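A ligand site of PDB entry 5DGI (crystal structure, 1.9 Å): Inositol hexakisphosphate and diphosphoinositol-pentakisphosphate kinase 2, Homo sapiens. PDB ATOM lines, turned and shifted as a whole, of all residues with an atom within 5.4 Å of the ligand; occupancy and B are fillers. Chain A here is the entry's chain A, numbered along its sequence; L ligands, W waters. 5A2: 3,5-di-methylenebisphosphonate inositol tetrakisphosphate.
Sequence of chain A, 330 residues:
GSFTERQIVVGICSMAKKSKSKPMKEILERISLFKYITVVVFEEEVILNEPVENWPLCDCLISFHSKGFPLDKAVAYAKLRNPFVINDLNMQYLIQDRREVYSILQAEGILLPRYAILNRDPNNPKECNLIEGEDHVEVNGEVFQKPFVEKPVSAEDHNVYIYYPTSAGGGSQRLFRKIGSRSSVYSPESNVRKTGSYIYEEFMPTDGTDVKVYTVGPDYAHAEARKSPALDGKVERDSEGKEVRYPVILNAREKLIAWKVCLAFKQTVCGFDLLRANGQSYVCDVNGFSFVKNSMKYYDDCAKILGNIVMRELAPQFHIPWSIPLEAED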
ATOM      1  N   LYS A  17       6.413  19.014   8.884  1.00  0.00           N
ATOM      2  CA  LYS A  17       5.218  19.255   8.058  1.00  0.00           C
ATOM      3  C   LYS A  17       5.302  20.625   7.359  1.00  0.00           C
ATOM      4  O   LYS A  17       4.849  20.784   6.229  1.00  0.00           O
ATOM      5  CB  LYS A  17       3.954  19.190   8.924  1.00  0.00           C
ATOM      6  CG  LYS A  17       2.655  19.101   8.139  1.00  0.00           C
ATOM      7  CD  LYS A  17       1.511  18.682   9.057  1.00  0.00           C
ATOM      8  CE  LYS A  17       0.155  19.036   8.461  1.00  0.00           C
ATOM      9  NZ  LYS A  17      -0.155  18.313   7.203  1.00  0.00           N
ATOM     10  N   LYS A  18       5.885  21.585   8.070  1.00  0.00           N
ATOM     11  CA  LYS A  18       6.066  22.936   7.532  1.00  0.00           C
ATOM     12  C   LYS A  18       7.356  23.068   6.722  1.00  0.00           C
ATOM     13  O   LYS A  18       7.345  23.662   5.640  1.00  0.00           O
ATOM     14  CB  LYS A  18       6.019  23.985   8.643  1.00  0.00           C
ATOM     15  CG  LYS A  18       4.743  23.953   9.508  1.00  0.00           C
ATOM     16  CD  LYS A  18       3.501  24.312   8.697  1.00  0.00           C
ATOM     17  CE  LYS A  18       2.259  24.317   9.583  1.00  0.00           C
ATOM     18  NZ  LYS A  18       0.994  24.424   8.793  1.00  0.00           N
ATOM     19  N   HIS A  65       6.158  28.816  14.946  1.00  0.00           N
ATOM     20  CA  HIS A  65       5.372  27.841  15.664  1.00  0.00           C
ATOM     21  C   HIS A  65       4.275  27.243  14.792  1.00  0.00           C
ATOM     22  O   HIS A  65       3.680  27.929  13.957  1.00  0.00           O
ATOM     23  CB  HIS A  65       4.771  28.472  16.913  1.00  0.00           C
ATOM     24  CG  HIS A  65       3.845  27.571  17.665  1.00  0.00           C
ATOM     25  ND1 HIS A  65       2.491  27.532  17.429  1.00  0.00           N
ATOM     26  CD2 HIS A  65       4.087  26.668  18.647  1.00  0.00           C
ATOM     27  CE1 HIS A  65       1.927  26.646  18.232  1.00  0.00           C
ATOM     28  NE2 HIS A  65       2.872  26.104  18.979  1.00  0.00           N
ATOM     29  N   SER A  66       4.052  25.945  14.972  1.00  0.00           N
ATOM     30  CA  SER A  66       2.855  25.246  14.523  1.00  0.00           C
ATOM     31  C   SER A  66       2.616  24.155  15.560  1.00  0.00           C
ATOM     32  O   SER A  66       3.395  24.024  16.505  1.00  0.00           O
ATOM     33  CB  SER A  66       3.053  24.666  13.113  1.00  0.00           C
ATOM     34  OG  SER A  66       4.098  23.723  13.084  1.00  0.00           O
ATOM     35  N   LYS A  67       1.533  23.388  15.408  1.00  0.00           N
ATOM     36  CA  LYS A  67       1.181  22.353  16.382  1.00  0.00           C
ATOM     37  C   LYS A  67       2.373  21.455  16.698  1.00  0.00           C
ATOM     38  O   LYS A  67       2.993  20.896  15.795  1.00  0.00           O
ATOM     39  CB  LYS A  67      -0.013  21.517  15.888  1.00  0.00           C
ATOM     40  CG  LYS A  67      -0.606  20.590  16.946  1.00  0.00           C
ATOM     41  CD  LYS A  67      -1.876  19.906  16.465  1.00  0.00           C
ATOM     42  CE  LYS A  67      -1.589  18.726  15.552  1.00  0.00           C
ATOM     43  NZ  LYS A  67      -2.826  17.945  15.253  1.00  0.00           N
ATOM     44  N   GLU A 156      -5.381  28.946  18.248  1.00  0.00           N
ATOM     45  CA  GLU A 156      -5.122  27.603  17.729  1.00  0.00           C
ATOM     46  C   GLU A 156      -6.421  26.792  17.633  1.00  0.00           C
ATOM     47  O   GLU A 156      -6.442  25.719  17.029  1.00  0.00           O
ATOM     48  CB  GLU A 156      -4.132  26.871  18.654  1.00  0.00           C
ATOM     49  CG  GLU A 156      -2.718  27.430  18.657  1.00  0.00           C
ATOM     50  CD  GLU A 156      -1.869  26.844  17.545  1.00  0.00           C
ATOM     51  OE1 GLU A 156      -1.947  27.350  16.399  1.00  0.00           O
ATOM     52  OE2 GLU A 156      -1.109  25.895  17.815  1.00  0.00           O
ATOM     53  N   HIS A 158     -10.006  26.573  16.147  1.00  0.00           N
ATOM     54  CA  HIS A 158     -10.713  27.106  14.980  1.00  0.00           C
ATOM     55  C   HIS A 158     -12.215  26.842  14.991  1.00  0.00           C
ATOM     56  O   HIS A 158     -12.917  27.028  13.991  1.00  0.00           O
ATOM     57  CB  HIS A 158     -10.030  26.576  13.710  1.00  0.00           C
ATOM     58  CG  HIS A 158      -8.567  26.892  13.659  1.00  0.00           C
ATOM     59  ND1 HIS A 158      -8.093  28.160  13.428  1.00  0.00           N
ATOM     60  CD2 HIS A 158      -7.476  26.114  13.882  1.00  0.00           C
ATOM     61  CE1 HIS A 158      -6.777  28.152  13.466  1.00  0.00           C
ATOM     62  NE2 HIS A 158      -6.374  26.916  13.743  1.00  0.00           N
ATOM     63  N   ARG A 177     -11.536  23.600  11.444  1.00  0.00           N
ATOM     64  CA  ARG A 177     -10.436  23.315  10.518  1.00  0.00           C
ATOM     65  C   ARG A 177     -11.006  22.493   9.371  1.00  0.00           C
ATOM     66  O   ARG A 177     -11.625  21.461   9.603  1.00  0.00           O
ATOM     67  CB  ARG A 177      -9.326  22.548  11.230  1.00  0.00           C
ATOM     68  CG  ARG A 177      -8.277  21.957  10.304  1.00  0.00           C
ATOM     69  CD  ARG A 177      -7.038  21.502  11.054  1.00  0.00           C
ATOM     70  NE  ARG A 177      -6.460  22.575  11.867  1.00  0.00           N
ATOM     71  CZ  ARG A 177      -5.691  23.550  11.403  1.00  0.00           C
ATOM     72  NH1 ARG A 177      -5.373  23.607  10.113  1.00  0.00           N
ATOM     73  NH2 ARG A 177      -5.234  24.476  12.230  1.00  0.00           N
ATOM     74  N   LYS A 178     -10.830  22.968   8.132  1.00  0.00           N
ATOM     75  CA  LYS A 178     -11.477  22.321   6.997  1.00  0.00           C
ATOM     76  C   LYS A 178     -10.979  20.883   6.832  1.00  0.00           C
ATOM     77  O   LYS A 178      -9.786  20.608   6.944  1.00  0.00           O
ATOM     78  CB  LYS A 178     -11.346  23.133   5.695  1.00  0.00           C
ATOM     79  CG  LYS A 178      -9.981  23.139   5.020  1.00  0.00           C
ATOM     80  CD  LYS A 178     -10.031  23.980   3.744  1.00  0.00           C
ATOM     81  CE  LYS A 178      -8.713  23.934   2.983  1.00  0.00           C
ATOM     82  NZ  LYS A 178      -7.609  24.625   3.698  1.00  0.00           N
ATOM     83  N   TYR A 214      -0.798  37.914   2.670  1.00  0.00           N
ATOM     84  CA  TYR A 214       0.474  37.278   2.982  1.00  0.00           C
ATOM     85  C   TYR A 214       1.601  38.282   2.766  1.00  0.00           C
ATOM     86  O   TYR A 214       1.911  38.638   1.622  1.00  0.00           O
ATOM     87  CB  TYR A 214       0.687  36.076   2.060  1.00  0.00           C
ATOM     88  CG  TYR A 214      -0.359  34.990   2.147  1.00  0.00           C
ATOM     89  CD1 TYR A 214      -1.591  35.122   1.506  1.00  0.00           C
ATOM     90  CD2 TYR A 214      -0.108  33.800   2.841  1.00  0.00           C
ATOM     91  CE1 TYR A 214      -2.543  34.117   1.553  1.00  0.00           C
ATOM     92  CE2 TYR A 214      -1.050  32.787   2.902  1.00  0.00           C
ATOM     93  CZ  TYR A 214      -2.264  32.956   2.268  1.00  0.00           C
ATOM     94  OH  TYR A 214      -3.205  31.942   2.315  1.00  0.00           O
ATOM     95  N   ARG A 226     -11.076  33.794  -0.803  1.00  0.00           N
ATOM     96  CA  ARG A 226     -11.691  32.466  -0.767  1.00  0.00           C
ATOM     97  C   ARG A 226     -13.098  32.587  -0.211  1.00  0.00           C
ATOM     98  O   ARG A 226     -13.368  33.498   0.576  1.00  0.00           O
ATOM     99  CB  ARG A 226     -10.864  31.494   0.073  1.00  0.00           C
ATOM    100  CG  ARG A 226      -9.479  31.193  -0.506  1.00  0.00           C
ATOM    101  CD  ARG A 226      -8.752  30.095   0.249  1.00  0.00           C
ATOM    102  NE  ARG A 226      -7.332  30.063  -0.097  1.00  0.00           N
ATOM    103  CZ  ARG A 226      -6.484  29.100   0.276  1.00  0.00           C
ATOM    104  NH1 ARG A 226      -6.918  28.073   1.005  1.00  0.00           N
ATOM    105  NH2 ARG A 226      -5.208  29.156  -0.093  1.00  0.00           N
ATOM    106  N   GLU A 243      -8.282  24.226  -3.182  1.00  0.00           N
ATOM    107  CA  GLU A 243      -9.369  25.161  -2.871  1.00  0.00           C
ATOM    108  C   GLU A 243      -9.364  26.343  -3.837  1.00  0.00           C
ATOM    109  O   GLU A 243      -8.320  26.929  -4.113  1.00  0.00           O
ATOM    110  CB  GLU A 243      -9.291  25.669  -1.432  1.00  0.00           C
ATOM    111  CG  GLU A 243     -10.508  26.501  -1.025  1.00  0.00           C
ATOM    112  CD  GLU A 243     -10.494  26.907   0.436  1.00  0.00           C
ATOM    113  OE1 GLU A 243      -9.467  26.711   1.125  1.00  0.00           O
ATOM    114  OE2 GLU A 243     -11.529  27.427   0.911  1.00  0.00           O
ATOM    115  N   ASN A 287      -2.230  35.357  11.760  1.00  0.00           N
ATOM    116  CA  ASN A 287      -1.752  33.982  11.897  1.00  0.00           C
ATOM    117  C   ASN A 287      -0.259  33.801  12.012  1.00  0.00           C
ATOM    118  O   ASN A 287       0.210  32.702  12.337  1.00  0.00           O
ATOM    119  CB  ASN A 287      -2.298  33.143  10.738  1.00  0.00           C
ATOM    120  CG  ASN A 287      -3.797  33.023  10.794  1.00  0.00           C
ATOM    121  OD1 ASN A 287      -4.335  32.828  11.867  1.00  0.00           O
ATOM    122  ND2 ASN A 287      -4.475  33.193   9.661  1.00  0.00           N
ATOM    123  N   PHE A 289       3.529  33.301  10.576  1.00  0.00           N
ATOM    124  CA  PHE A 289       4.225  32.751   9.407  1.00  0.00           C
ATOM    125  C   PHE A 289       3.319  31.908   8.537  1.00  0.00           C
ATOM    126  O   PHE A 289       2.741  30.908   8.996  1.00  0.00           O
ATOM    127  CB  PHE A 289       5.427  31.918   9.856  1.00  0.00           C
ATOM    128  CG  PHE A 289       6.424  31.644   8.770  1.00  0.00           C
ATOM    129  CD1 PHE A 289       6.183  30.665   7.799  1.00  0.00           C
ATOM    130  CD2 PHE A 289       7.604  32.368   8.707  1.00  0.00           C
ATOM    131  CE1 PHE A 289       7.118  30.410   6.794  1.00  0.00           C
ATOM    132  CE2 PHE A 289       8.551  32.117   7.710  1.00  0.00           C
ATOM    133  CZ  PHE A 289       8.302  31.143   6.760  1.00  0.00           C
ATOM    134  N   SER A 290       3.207  32.292   7.273  1.00  0.00           N
ATOM    135  CA  SER A 290       2.403  31.572   6.297  1.00  0.00           C
ATOM    136  C   SER A 290       2.823  31.973   4.894  1.00  0.00           C
ATOM    137  O   SER A 290       2.976  33.161   4.600  1.00  0.00           O
ATOM    138  CB  SER A 290       0.914  31.861   6.490  1.00  0.00           C
ATOM    139  OG  SER A 290       0.125  30.973   5.725  1.00  0.00           O
ATOM    140  N   PHE A 291       3.015  30.970   4.035  1.00  0.00           N
ATOM    141  CA  PHE A 291       3.361  31.178   2.627  1.00  0.00           C
ATOM    142  C   PHE A 291       2.105  31.046   1.775  1.00  0.00           C
ATOM    143  O   PHE A 291       1.202  30.300   2.134  1.00  0.00           O
ATOM    144  CB  PHE A 291       4.357  30.123   2.147  1.00  0.00           C
ATOM    145  CG  PHE A 291       5.774  30.314   2.629  1.00  0.00           C
ATOM    146  CD1 PHE A 291       6.310  31.587   2.811  1.00  0.00           C
ATOM    147  CD2 PHE A 291       6.589  29.216   2.850  1.00  0.00           C
ATOM    148  CE1 PHE A 291       7.620  31.754   3.225  1.00  0.00           C
ATOM    149  CE2 PHE A 291       7.898  29.371   3.272  1.00  0.00           C
ATOM    150  CZ  PHE A 291       8.423  30.640   3.460  1.00  0.00           C
ATOM    151  N   LYS A 293       0.213  29.417  -1.260  1.00  0.00           N
ATOM    152  CA  LYS A 293       0.312  28.087  -1.829  1.00  0.00           C
ATOM    153  C   LYS A 293       0.044  28.153  -3.331  1.00  0.00           C
ATOM    154  O   LYS A 293      -0.811  28.913  -3.776  1.00  0.00           O
ATOM    155  CB  LYS A 293      -0.680  27.122  -1.156  1.00  0.00           C
ATOM    156  CG  LYS A 293      -0.338  26.736   0.274  1.00  0.00           C
ATOM    157  CD  LYS A 293      -0.779  27.793   1.275  1.00  0.00           C
ATOM    158  CE  LYS A 293      -0.351  27.443   2.701  1.00  0.00           C
ATOM    159  NZ  LYS A 293      -0.518  28.600   3.620  1.00  0.00           N
HETATM  160  C1  5A2 L   1      -3.463  26.760   5.919  1.00  0.00           C
HETATM  161  C2  5A2 L   1      -2.547  26.655   7.153  1.00  0.00           C
HETATM  162  C3  5A2 L   1      -2.952  25.449   8.023  1.00  0.00           C
HETATM  163  C4  5A2 L   1      -2.846  24.152   7.199  1.00  0.00           C
HETATM  164  C5  5A2 L   1      -3.763  24.221   5.987  1.00  0.00           C
HETATM  165  C6  5A2 L   1      -3.451  25.443   5.112  1.00  0.00           C
HETATM  166  O55 5A2 L   1      -2.937  18.629   6.062  1.00  0.00           O
HETATM  167  PB5 5A2 L   1      -3.206  19.637   5.019  1.00  0.00           P
HETATM  168  O65 5A2 L   1      -2.026  20.530   4.909  1.00  0.00           O
HETATM  169  O75 5A2 L   1      -3.716  18.943   3.814  1.00  0.00           O
HETATM  170  C5B 5A2 L   1      -4.577  20.588   5.734  1.00  0.00           C
HETATM  171  PA5 5A2 L   1      -4.869  22.101   4.780  1.00  0.00           P
HETATM  172  O35 5A2 L   1      -6.113  22.743   5.270  1.00  0.00           O
HETATM  173  O25 5A2 L   1      -4.722  21.777   3.338  1.00  0.00           O
HETATM  174  O15 5A2 L   1      -3.602  23.020   5.197  1.00  0.00           O
HETATM  175  O14 5A2 L   1      -3.254  23.033   7.995  1.00  0.00           O
HETATM  176  PA4 5A2 L   1      -2.226  21.945   8.629  1.00  0.00           P
HETATM  177  O34 5A2 L   1      -0.765  22.347   8.101  1.00  0.00           O
HETATM  178  O44 5A2 L   1      -2.567  20.619   8.075  1.00  0.00           O
HETATM  179  O24 5A2 L   1      -2.269  22.122  10.094  1.00  0.00           O
HETATM  180  O16 5A2 L   1      -4.464  25.507   4.101  1.00  0.00           O
HETATM  181  PA6 5A2 L   1      -4.104  25.498   2.531  1.00  0.00           P
HETATM  182  O36 5A2 L   1      -3.996  26.925   2.193  1.00  0.00           O
HETATM  183  O46 5A2 L   1      -2.859  24.708   2.407  1.00  0.00           O
HETATM  184  O26 5A2 L   1      -5.321  24.825   2.003  1.00  0.00           O
HETATM  185  O11 5A2 L   1      -2.989  27.832   5.063  1.00  0.00           O
HETATM  186  PA1 5A2 L   1      -3.875  29.139   4.719  1.00  0.00           P
HETATM  187  O41 5A2 L   1      -4.385  29.620   6.012  1.00  0.00           O
HETATM  188  O21 5A2 L   1      -2.922  30.033   4.025  1.00  0.00           O
HETATM  189  O31 5A2 L   1      -4.942  28.605   3.831  1.00  0.00           O
HETATM  190  O12 5A2 L   1      -1.175  26.521   6.723  1.00  0.00           O
HETATM  191  PA2 5A2 L   1       0.006  27.525   7.112  1.00  0.00           P
HETATM  192  O42 5A2 L   1       0.530  26.962   8.372  1.00  0.00           O
HETATM  193  O22 5A2 L   1       0.868  27.432   5.936  1.00  0.00           O
HETATM  194  O32 5A2 L   1      -0.654  28.832   7.289  1.00  0.00           O
HETATM  195  O13 5A2 L   1      -2.096  25.373   9.183  1.00  0.00           O
HETATM  196  PA3 5A2 L   1      -2.379  26.246  10.538  1.00  0.00           P
HETATM  197  O23 5A2 L   1      -3.910  26.783  10.473  1.00  0.00           O
HETATM  198  O33 5A2 L   1      -1.424  27.371  10.658  1.00  0.00           O
HETATM  199  C3B 5A2 L   1      -2.285  25.044  11.891  1.00  0.00           C
HETATM  200  PB3 5A2 L   1      -0.614  24.529  12.173  1.00  0.00           P
HETATM  201  O53 5A2 L   1       0.220  25.678  11.777  1.00  0.00           O
HETATM  202  O63 5A2 L   1      -0.608  24.196  13.608  1.00  0.00           O
HETATM  203  O73 5A2 L   1      -0.483  23.373  11.267  1.00  0.00           O
HETATM  204  O   HOH W   1      -3.735  29.753  10.329  1.00  0.00           O
HETATM  205  O   HOH W   2       0.090  28.520  12.381  1.00  0.00           O
HETATM  206  O   HOH W   3      -3.664  27.224  14.117  1.00  0.00           O
HETATM  207  O   HOH W   4       0.781  20.957  11.381  1.00  0.00           O
HETATM  208  O   HOH W   5      -6.069  31.463   4.234  1.00  0.00           O
HETATM  209  O   HOH W   6       0.215  29.739  10.004  1.00  0.00           O
HETATM  210  O   HOH W   7       2.238  27.706  11.449  1.00  0.00           O
HETATM  211  O   HOH W   8      -2.610  30.501   7.997  1.00  0.00           O
HETATM  212  O   HOH W   9       3.028  28.030   8.903  1.00  0.00           O
HETATM  213  O   HOH W  10      -0.082  27.053  14.397  1.00  0.00           O
HETATM  214  O   HOH W  11      -2.266  29.529  12.654  1.00  0.00           O
HETATM  215  O   HOH W  12       3.116  28.345   4.974  1.00  0.00           O
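Water W12 bridges O22 of the ligand and N of Phe 291. Water W9 bridges O42 of the ligand (2.8 Å) and O of Phe 289 (2.9 Å). Water W7 lies within hydrogen-bond range of an oxygen (O53) of the ligand (2.9 Å) and the backbone carbonyl oxygen (O) of His 65 (2.9 Å). Water W6 bridges O33 of the ligand (3.0 Å) and O of Phe 289 (3.0 Å). Water W10 bridges OE1 of Glu 156 and O53 of the ligand. Water W3 bridges a ring nitrogen (NE2) of His 158 and the side-chain carboxylate of Glu 156.
An oxygen (O26) of the ligand is in salt-bridge range of the side-chain amino group (NZ) of Lys 178, 2.9 Å away. O55 of the ligand is in salt-bridge range of NZ of Lys 17. The guanidinium group of Arg 177 is in salt-bridge range of an oxygen (O23) of the ligand (3.2 Å). The side-chain amino group (NZ) of Lys 18 lies within salt-bridge range of an oxygen (O42) of the ligand (2.6 Å). An oxygen (O21) of the ligand is in salt-bridge range of the side-chain amino group (NZ) of Lys 293 (2.8 Å). The side-chain hydroxyl (OH) of Tyr 214 lies within hydrogen-bond range of an oxygen (O21) of the ligand. The side-chain hydroxyl (OG) of Ser 290 lies within hydrogen-bond range of an oxygen (O32) of the ligand (2.8 Å). The guanidinium group of Arg 226 lies within salt-bridge range of an oxygen (O36) of the ligand (3.4 Å). The backbone NH (N) of Lys 67 sits at hydrogen-bond distance from an oxygen (O63) of the ligand, 2.9 Å away.
NZ of Lys 293 is in hydrogen-bond range of OG of Ser 290. NZ of Lys 293 is in hydrogen-bond range of O of Phe 291, at 2.8 Å. The guanidinium group (NH1) of Arg 226 lies within salt-bridge range of the side-chain carboxylate (OE1) of Glu 243 (2.9 Å). NZ of Lys 178 lies within salt-bridge range of OE1 of Glu 243 (3.8 Å). NH2 of Arg 177 lies within hydrogen-bond range of NE2 of His 158 (3.1 Å).
Residues that only touch the ligand: Ser 66. Hydrophobic or aromatic side chains within 4 Å of the ligand: Tyr 214. The nearest printed residue that does not touch the ligand is His 158 (4.1 Å).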
